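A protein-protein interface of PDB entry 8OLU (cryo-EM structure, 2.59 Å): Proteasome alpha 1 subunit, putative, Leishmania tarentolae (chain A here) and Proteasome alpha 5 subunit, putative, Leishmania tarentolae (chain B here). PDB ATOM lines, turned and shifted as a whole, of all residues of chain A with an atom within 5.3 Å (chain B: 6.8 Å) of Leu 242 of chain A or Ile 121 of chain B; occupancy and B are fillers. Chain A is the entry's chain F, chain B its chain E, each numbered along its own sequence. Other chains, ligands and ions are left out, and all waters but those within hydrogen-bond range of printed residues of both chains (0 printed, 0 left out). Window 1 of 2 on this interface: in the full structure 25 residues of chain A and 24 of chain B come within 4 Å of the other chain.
Ala 192 of chain A touches Gly 119 of chain B (CB to O, 3.4 Å). CE1 of Phe 115 of chain B touches CD1 of Leu 242 of chain A (3.8 Å). Leu 242 of chain A touches Ile 121 of chain B (CD1 to CG1, 3.96 Å). Ala 244 of chain A touches Ser 259 of chain B. O of Asn 113 of chain B touches CB of Arg 291 of chain A (3.3 Å). Arg 291 of chain A touches Phe 115 of chain B. CD1 of Ile 121 of chain B touches NE of Arg 291 of chain A, at 3.0 Å. Gly 294 of chain A touches Phe 115 of chain B (CA to CZ, 3.9 Å).
OD2 of Asp 245 of chain A lies within salt-bridge range of NH1 of Arg 291 of chain A (2.5 Å). O of Gly 294 of chain A is in hydrogen-bond range of N of Leu 242 of chain A (2.9 Å). N of Gly 294 of chain A sits at hydrogen-bond distance from OD2 of Asp 245 of chain A (2.9 Å).
Of chain B, only Phe 115 and Ile 121 come within 4 Å of Leu 242 of chain A. Ile 121 of chain B touches just these residues of chain A: Leu 242 and Arg 291. Printed residues of chain A within 4 Å of Ser 259 of chain B: Ala 244. Printed residues of chain B within 4 Å of Ala 244 of chain A: Ser 259. Of the printed residues of chain B, Arg 291 of chain A touches Asn 113, Phe 115 and Ile 121. Printed residues of chain A within 4 Å of Asn 113 of chain B: Arg 291. Of the printed residues of chain B, Ala 192 of chain A touches Gly 119 (3.4 Å). Val 295 of chain A touches none of the printed residues of chain B. Ile 124 of chain B touches none of the printed residues of chain A. The nearest printed residue of chain B that does not touch Ala 244 of chain A is Thr 261 of chain B (4.7 Å).
Hydrophobic or aromatic side chains of chain B within 4 Å of the printed part of chain A: Phe 115 and Ile 121. Along chain B the printed residues that touch a printed residue of chain A span positions 113 to 259. Of the 12 printed residues of chain A, 5 touch a printed residue of chain B. Printed residues of chain A that touch a printed residue of chain B: Ala 192, Leu 242, Ala 244, Arg 291 and Gly 294. Among the printed residues, 8 pairs touch across the chains. Among the printed residues, no Asp or Glu carboxylate lies within 4 Å of a Lys or Arg side-chain nitrogen of the other chain.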
ATOM      1  N   ALA A 192       5.571  32.931 -11.314  1.00  0.00           N
ATOM      2  CA  ALA A 192       6.447  31.788 -11.472  1.00  0.00           C
ATOM      3  C   ALA A 192       7.889  32.228 -11.523  1.00  0.00           C
ATOM      4  O   ALA A 192       8.776  31.482 -11.134  1.00  0.00           O
ATOM      5  CB  ALA A 192       6.132  31.058 -12.747  1.00  0.00           C
ATOM      6  N   ILE A 239      17.923  30.789 -16.690  1.00  0.00           N
ATOM      7  CA  ILE A 239      16.493  30.913 -16.529  1.00  0.00           C
ATOM      8  C   ILE A 239      16.086  30.936 -15.086  1.00  0.00           C
ATOM      9  O   ILE A 239      16.710  30.330 -14.243  1.00  0.00           O
ATOM     10  CB  ILE A 239      15.802  29.720 -17.145  1.00  0.00           C
ATOM     11  CG1 ILE A 239      16.014  28.523 -16.244  1.00  0.00           C
ATOM     12  CG2 ILE A 239      16.264  29.453 -18.561  1.00  0.00           C
ATOM     13  CD1 ILE A 239      15.500  27.262 -16.895  1.00  0.00           C
ATOM     14  N   SER A 240      14.915  31.486 -14.872  1.00  0.00           N
ATOM     15  CA  SER A 240      14.265  31.397 -13.586  1.00  0.00           C
ATOM     16  C   SER A 240      12.779  31.161 -13.796  1.00  0.00           C
ATOM     17  O   SER A 240      12.164  31.761 -14.657  1.00  0.00           O
ATOM     18  CB  SER A 240      14.529  32.607 -12.724  1.00  0.00           C
ATOM     19  OG  SER A 240      13.294  33.205 -12.355  1.00  0.00           O
ATOM     20  N   GLY A 241      12.225  30.293 -12.968  1.00  0.00           N
ATOM     21  CA  GLY A 241      10.827  29.946 -13.042  1.00  0.00           C
ATOM     22  C   GLY A 241      10.716  28.488 -13.426  1.00  0.00           C
ATOM     23  O   GLY A 241      11.547  27.689 -13.030  1.00  0.00           O
ATOM     24  N   LEU A 242       9.724  28.183 -14.236  1.00  0.00           N
ATOM     25  CA  LEU A 242       9.405  26.821 -14.560  1.00  0.00           C
ATOM     26  C   LEU A 242      10.457  26.259 -15.482  1.00  0.00           C
ATOM     27  O   LEU A 242      10.439  26.434 -16.687  1.00  0.00           O
ATOM     28  CB  LEU A 242       8.055  26.746 -15.266  1.00  0.00           C
ATOM     29  CG  LEU A 242       6.850  27.200 -14.451  1.00  0.00           C
ATOM     30  CD1 LEU A 242       5.606  26.826 -15.246  1.00  0.00           C
ATOM     31  CD2 LEU A 242       6.868  26.607 -13.028  1.00  0.00           C
ATOM     32  N   VAL A 243      11.286  25.440 -14.901  1.00  0.00           N
ATOM     33  CA  VAL A 243      12.439  24.969 -15.609  1.00  0.00           C
ATOM     34  C   VAL A 243      12.047  24.280 -16.900  1.00  0.00           C
ATOM     35  O   VAL A 243      12.815  24.324 -17.847  1.00  0.00           O
ATOM     36  CB  VAL A 243      13.214  24.032 -14.689  1.00  0.00           C
ATOM     37  CG1 VAL A 243      14.384  23.414 -15.413  1.00  0.00           C
ATOM     38  CG2 VAL A 243      13.642  24.806 -13.461  1.00  0.00           C
ATOM     39  N   ALA A 244      10.938  23.575 -16.916  1.00  0.00           N
ATOM     40  CA  ALA A 244      10.609  22.856 -18.126  1.00  0.00           C
ATOM     41  C   ALA A 244      10.309  23.821 -19.259  1.00  0.00           C
ATOM     42  O   ALA A 244      10.535  23.490 -20.416  1.00  0.00           O
ATOM     43  CB  ALA A 244       9.421  21.964 -17.908  1.00  0.00           C
ATOM     44  N   ASP A 245       9.744  24.987 -18.946  1.00  0.00           N
ATOM     45  CA  ASP A 245       9.575  26.002 -19.967  1.00  0.00           C
ATOM     46  C   ASP A 245      10.944  26.506 -20.418  1.00  0.00           C
ATOM     47  O   ASP A 245      11.203  26.658 -21.589  1.00  0.00           O
ATOM     48  CB  ASP A 245       8.612  27.077 -19.470  1.00  0.00           C
ATOM     49  CG  ASP A 245       7.191  26.532 -19.288  1.00  0.00           C
ATOM     50  OD1 ASP A 245       6.994  25.287 -19.516  1.00  0.00           O
ATOM     51  OD2 ASP A 245       6.269  27.349 -18.921  1.00  0.00           O
ATOM     52  N   GLY A 246      11.828  26.794 -19.484  1.00  0.00           N
ATOM     53  CA  GLY A 246      13.210  27.014 -19.833  1.00  0.00           C
ATOM     54  C   GLY A 246      13.644  26.069 -20.933  1.00  0.00           C
ATOM     55  O   GLY A 246      14.140  26.517 -21.941  1.00  0.00           O
ATOM     56  N   ARG A 291      -0.405  28.465 -23.099  1.00  0.00           N
ATOM     57  CA  ARG A 291      -0.306  29.268 -21.902  1.00  0.00           C
ATOM     58  C   ARG A 291       1.023  29.990 -21.939  1.00  0.00           C
ATOM     59  O   ARG A 291       1.958  29.597 -22.644  1.00  0.00           O
ATOM     60  CB  ARG A 291      -0.398  28.417 -20.648  1.00  0.00           C
ATOM     61  CG  ARG A 291       0.631  27.297 -20.620  1.00  0.00           C
ATOM     62  CD  ARG A 291       1.002  26.911 -19.196  1.00  0.00           C
ATOM     63  NE  ARG A 291       1.978  25.831 -19.253  1.00  0.00           N
ATOM     64  CZ  ARG A 291       3.265  25.965 -18.953  1.00  0.00           C
ATOM     65  NH1 ARG A 291       3.779  27.171 -18.702  1.00  0.00           N
ATOM     66  NH2 ARG A 291       4.022  24.879 -18.902  1.00  0.00           N
ATOM     67  N   GLY A 294       6.254  30.165 -18.073  1.00  0.00           N
ATOM     68  CA  GLY A 294       6.367  30.608 -16.709  1.00  0.00           C
ATOM     69  C   GLY A 294       7.829  30.767 -16.368  1.00  0.00           C
ATOM     70  O   GLY A 294       8.241  30.402 -15.282  1.00  0.00           O
ATOM     71  N   VAL A 295       8.592  31.329 -17.297  1.00  0.00           N
ATOM     72  CA  VAL A 295      10.021  31.368 -17.101  1.00  0.00           C
ATOM     73  C   VAL A 295      10.565  32.693 -17.576  1.00  0.00           C
ATOM     74  O   VAL A 295      10.093  33.252 -18.543  1.00  0.00           O
ATOM     75  CB  VAL A 295      10.633  30.204 -17.869  1.00  0.00           C
ATOM     76  CG1 VAL A 295      10.629  30.412 -19.373  1.00  0.00           C
ATOM     77  CG2 VAL A 295      12.041  29.937 -17.381  1.00  0.00           C
ATOM     78  N   VAL B 112      -6.623  23.292 -18.119  1.00  0.00           N
ATOM     79  CA  VAL B 112      -5.549  22.467 -17.584  1.00  0.00           C
ATOM     80  C   VAL B 112      -4.170  23.126 -17.710  1.00  0.00           C
ATOM     81  O   VAL B 112      -3.175  22.686 -17.120  1.00  0.00           O
ATOM     82  CB  VAL B 112      -5.558  21.115 -18.311  1.00  0.00           C
ATOM     83  CG1 VAL B 112      -6.868  20.383 -18.039  1.00  0.00           C
ATOM     84  CG2 VAL B 112      -5.269  21.261 -19.806  1.00  0.00           C
ATOM     85  N   ASN B 113      -4.154  24.188 -18.515  1.00  0.00           N
ATOM     86  CA  ASN B 113      -2.986  24.986 -18.787  1.00  0.00           C
ATOM     87  C   ASN B 113      -3.017  26.252 -17.944  1.00  0.00           C
ATOM     88  O   ASN B 113      -2.444  27.254 -18.287  1.00  0.00           O
ATOM     89  CB  ASN B 113      -3.021  25.367 -20.267  1.00  0.00           C
ATOM     90  CG  ASN B 113      -2.159  24.491 -21.144  1.00  0.00           C
ATOM     91  OD1 ASN B 113      -1.461  23.591 -20.664  1.00  0.00           O
ATOM     92  ND2 ASN B 113      -2.210  24.797 -22.432  1.00  0.00           N
ATOM     93  N   THR B 114      -3.693  26.225 -16.831  1.00  0.00           N
ATOM     94  CA  THR B 114      -3.946  27.450 -16.128  1.00  0.00           C
ATOM     95  C   THR B 114      -2.931  27.638 -15.019  1.00  0.00           C
ATOM     96  O   THR B 114      -2.640  26.671 -14.328  1.00  0.00           O
ATOM     97  CB  THR B 114      -5.344  27.386 -15.526  1.00  0.00           C
ATOM     98  OG1 THR B 114      -6.157  27.388 -16.694  1.00  0.00           O
ATOM     99  CG2 THR B 114      -5.607  28.522 -14.563  1.00  0.00           C
ATOM    100  N   PHE B 115      -2.476  28.864 -14.821  1.00  0.00           N
ATOM    101  CA  PHE B 115      -1.655  29.157 -13.669  1.00  0.00           C
ATOM    102  C   PHE B 115      -2.513  29.557 -12.498  1.00  0.00           C
ATOM    103  O   PHE B 115      -3.478  30.277 -12.675  1.00  0.00           O
ATOM    104  CB  PHE B 115      -0.722  30.344 -13.855  1.00  0.00           C
ATOM    105  CG  PHE B 115       0.458  30.044 -14.717  1.00  0.00           C
ATOM    106  CD1 PHE B 115       1.646  29.652 -14.156  1.00  0.00           C
ATOM    107  CD2 PHE B 115       0.380  30.202 -16.082  1.00  0.00           C
ATOM    108  CE1 PHE B 115       2.711  29.304 -14.960  1.00  0.00           C
ATOM    109  CE2 PHE B 115       1.447  29.901 -16.904  1.00  0.00           C
ATOM    110  CZ  PHE B 115       2.621  29.466 -16.337  1.00  0.00           C
ATOM    111  N   SER B 116      -2.070  29.140 -11.311  1.00  0.00           N
ATOM    112  CA  SER B 116      -2.540  29.663 -10.041  1.00  0.00           C
ATOM    113  C   SER B 116      -1.971  31.045  -9.822  1.00  0.00           C
ATOM    114  O   SER B 116      -0.987  31.420 -10.458  1.00  0.00           O
ATOM    115  CB  SER B 116      -2.116  28.779  -8.903  1.00  0.00           C
ATOM    116  OG  SER B 116      -0.691  28.745  -8.664  1.00  0.00           O
ATOM    117  N   GLY B 119       1.809  31.162  -9.356  1.00  0.00           N
ATOM    118  CA  GLY B 119       2.686  30.871 -10.470  1.00  0.00           C
ATOM    119  C   GLY B 119       2.939  29.388 -10.666  1.00  0.00           C
ATOM    120  O   GLY B 119       3.932  28.995 -11.271  1.00  0.00           O
ATOM    121  N   ARG B 120       1.999  28.578 -10.205  1.00  0.00           N
ATOM    122  CA  ARG B 120       2.087  27.150 -10.405  1.00  0.00           C
ATOM    123  C   ARG B 120       0.947  26.760 -11.306  1.00  0.00           C
ATOM    124  O   ARG B 120      -0.113  27.339 -11.229  1.00  0.00           O
ATOM    125  CB  ARG B 120       2.036  26.455  -9.049  1.00  0.00           C
ATOM    126  CG  ARG B 120       3.294  26.732  -8.247  1.00  0.00           C
ATOM    127  CD  ARG B 120       3.411  25.977  -6.940  1.00  0.00           C
ATOM    128  NE  ARG B 120       3.898  26.870  -5.887  1.00  0.00           N
ATOM    129  CZ  ARG B 120       3.135  27.381  -4.920  1.00  0.00           C
ATOM    130  NH1 ARG B 120       1.828  27.176  -4.889  1.00  0.00           N
ATOM    131  NH2 ARG B 120       3.697  28.111  -3.974  1.00  0.00           N
ATOM    132  N   ILE B 121       1.217  25.838 -12.197  1.00  0.00           N
ATOM    133  CA  ILE B 121       0.191  25.238 -13.006  1.00  0.00           C
ATOM    134  C   ILE B 121      -0.545  24.254 -12.119  1.00  0.00           C
ATOM    135  O   ILE B 121       0.076  23.384 -11.529  1.00  0.00           O
ATOM    136  CB  ILE B 121       0.868  24.497 -14.156  1.00  0.00           C
ATOM    137  CG1 ILE B 121       1.950  25.346 -14.847  1.00  0.00           C
ATOM    138  CG2 ILE B 121      -0.142  23.891 -15.121  1.00  0.00           C
ATOM    139  CD1 ILE B 121       1.570  25.863 -16.232  1.00  0.00           C
ATOM    140  N   PHE B 122      -1.875  24.370 -12.061  1.00  0.00           N
ATOM    141  CA  PHE B 122      -2.698  23.570 -11.175  1.00  0.00           C
ATOM    142  C   PHE B 122      -2.635  22.077 -11.470  1.00  0.00           C
ATOM    143  O   PHE B 122      -2.508  21.263 -10.580  1.00  0.00           O
ATOM    144  CB  PHE B 122      -4.122  24.034 -11.360  1.00  0.00           C
ATOM    145  CG  PHE B 122      -4.470  25.284 -10.597  1.00  0.00           C
ATOM    146  CD1 PHE B 122      -4.386  25.303  -9.202  1.00  0.00           C
ATOM    147  CD2 PHE B 122      -4.884  26.438 -11.269  1.00  0.00           C
ATOM    148  CE1 PHE B 122      -4.777  26.426  -8.502  1.00  0.00           C
ATOM    149  CE2 PHE B 122      -5.235  27.573 -10.558  1.00  0.00           C
ATOM    150  CZ  PHE B 122      -5.183  27.554  -9.183  1.00  0.00           C
ATOM    151  N   GLN B 123      -2.771  21.667 -12.700  1.00  0.00           N
ATOM    152  CA  GLN B 123      -2.737  20.249 -12.922  1.00  0.00           C
ATOM    153  C   GLN B 123      -1.372  19.696 -12.530  1.00  0.00           C
ATOM    154  O   GLN B 123      -1.301  18.525 -12.180  1.00  0.00           O
ATOM    155  CB  GLN B 123      -3.021  19.884 -14.380  1.00  0.00           C
ATOM    156  CG  GLN B 123      -4.484  20.046 -14.765  1.00  0.00           C
ATOM    157  CD  GLN B 123      -5.395  19.172 -13.950  1.00  0.00           C
ATOM    158  OE1 GLN B 123      -5.496  17.971 -14.190  1.00  0.00           O
ATOM    159  NE2 GLN B 123      -6.021  19.775 -12.957  1.00  0.00           N
ATOM    160  N   ILE B 124      -0.286  20.475 -12.625  1.00  0.00           N
ATOM    161  CA  ILE B 124       0.988  19.948 -12.187  1.00  0.00           C
ATOM    162  C   ILE B 124       0.961  19.776 -10.673  1.00  0.00           C
ATOM    163  O   ILE B 124       1.445  18.787 -10.169  1.00  0.00           O
ATOM    164  CB  ILE B 124       2.173  20.827 -12.583  1.00  0.00           C
ATOM    165  CG1 ILE B 124       2.319  20.999 -14.086  1.00  0.00           C
ATOM    166  CG2 ILE B 124       3.456  20.301 -11.990  1.00  0.00           C
ATOM    167  CD1 ILE B 124       2.468  19.708 -14.794  1.00  0.00           C
ATOM    168  N   GLU B 125       0.417  20.725  -9.936  1.00  0.00           N
ATOM    169  CA  GLU B 125       0.488  20.636  -8.497  1.00  0.00           C
ATOM    170  C   GLU B 125      -0.325  19.460  -7.999  1.00  0.00           C
ATOM    171  O   GLU B 125       0.030  18.818  -7.013  1.00  0.00           O
ATOM    172  CB  GLU B 125       0.012  21.939  -7.880  1.00  0.00           C
ATOM    173  CG  GLU B 125       1.029  23.037  -8.103  1.00  0.00           C
ATOM    174  CD  GLU B 125       2.484  22.758  -7.688  1.00  0.00           C
ATOM    175  OE1 GLU B 125       2.840  22.998  -6.484  1.00  0.00           O
ATOM    176  OE2 GLU B 125       3.282  22.308  -8.573  1.00  0.00           O
ATOM    177  N   TYR B 126      -1.424  19.215  -8.704  1.00  0.00           N
ATOM    178  CA  TYR B 126      -2.276  18.089  -8.411  1.00  0.00           C
ATOM    179  C   TYR B 126      -1.574  16.811  -8.843  1.00  0.00           C
ATOM    180  O   TYR B 126      -1.452  15.886  -8.095  1.00  0.00           O
ATOM    181  CB  TYR B 126      -3.626  18.261  -9.110  1.00  0.00           C
ATOM    182  CG  TYR B 126      -4.428  19.508  -8.811  1.00  0.00           C
ATOM    183  CD1 TYR B 126      -4.222  20.301  -7.677  1.00  0.00           C
ATOM    184  CD2 TYR B 126      -5.414  19.911  -9.704  1.00  0.00           C
ATOM    185  CE1 TYR B 126      -4.979  21.452  -7.460  1.00  0.00           C
ATOM    186  CE2 TYR B 126      -6.148  21.082  -9.513  1.00  0.00           C
ATOM    187  CZ  TYR B 126      -5.924  21.859  -8.395  1.00  0.00           C
ATOM    188  OH  TYR B 126      -6.710  22.985  -8.264  1.00  0.00           O
ATOM    189  N   PHE B 223       1.106  18.293 -22.776  1.00  0.00           N
ATOM    190  CA  PHE B 223      -0.266  18.207 -22.273  1.00  0.00           C
ATOM    191  C   PHE B 223      -1.036  19.531 -22.491  1.00  0.00           C
ATOM    192  O   PHE B 223      -0.504  20.629 -22.297  1.00  0.00           O
ATOM    193  CB  PHE B 223      -0.278  17.640 -20.835  1.00  0.00           C
ATOM    194  CG  PHE B 223       0.223  18.534 -19.722  1.00  0.00           C
ATOM    195  CD1 PHE B 223      -0.648  19.417 -19.079  1.00  0.00           C
ATOM    196  CD2 PHE B 223       1.554  18.484 -19.314  1.00  0.00           C
ATOM    197  CE1 PHE B 223      -0.189  20.264 -18.082  1.00  0.00           C
ATOM    198  CE2 PHE B 223       2.015  19.338 -18.322  1.00  0.00           C
ATOM    199  CZ  PHE B 223       1.143  20.228 -17.713  1.00  0.00           C
ATOM    200  N   SER B 259       5.948  18.089 -13.812  1.00  0.00           N
ATOM    201  CA  SER B 259       6.444  19.338 -14.391  1.00  0.00           C
ATOM    202  C   SER B 259       7.187  19.068 -15.696  1.00  0.00           C
ATOM    203  O   SER B 259       6.967  19.768 -16.677  1.00  0.00           O
ATOM    204  CB  SER B 259       7.345  20.000 -13.394  1.00  0.00           C
ATOM    205  OG  SER B 259       7.096  19.519 -12.056  1.00  0.00           O
ATOM    206  N   THR B 261      10.583  18.364 -15.063  1.00  0.00           N
ATOM    207  CA  THR B 261      11.842  18.894 -14.595  1.00  0.00           C
ATOM    208  C   THR B 261      12.662  17.780 -13.967  1.00  0.00           C
ATOM    209  O   THR B 261      12.402  17.357 -12.829  1.00  0.00           O
ATOM    210  CB  THR B 261      11.696  20.055 -13.596  1.00  0.00           C
ATOM    211  OG1 THR B 261      12.913  20.090 -12.842  1.00  0.00           O
ATOM    212  CG2 THR B 261      10.566  19.953 -12.587  1.00  0.00           C
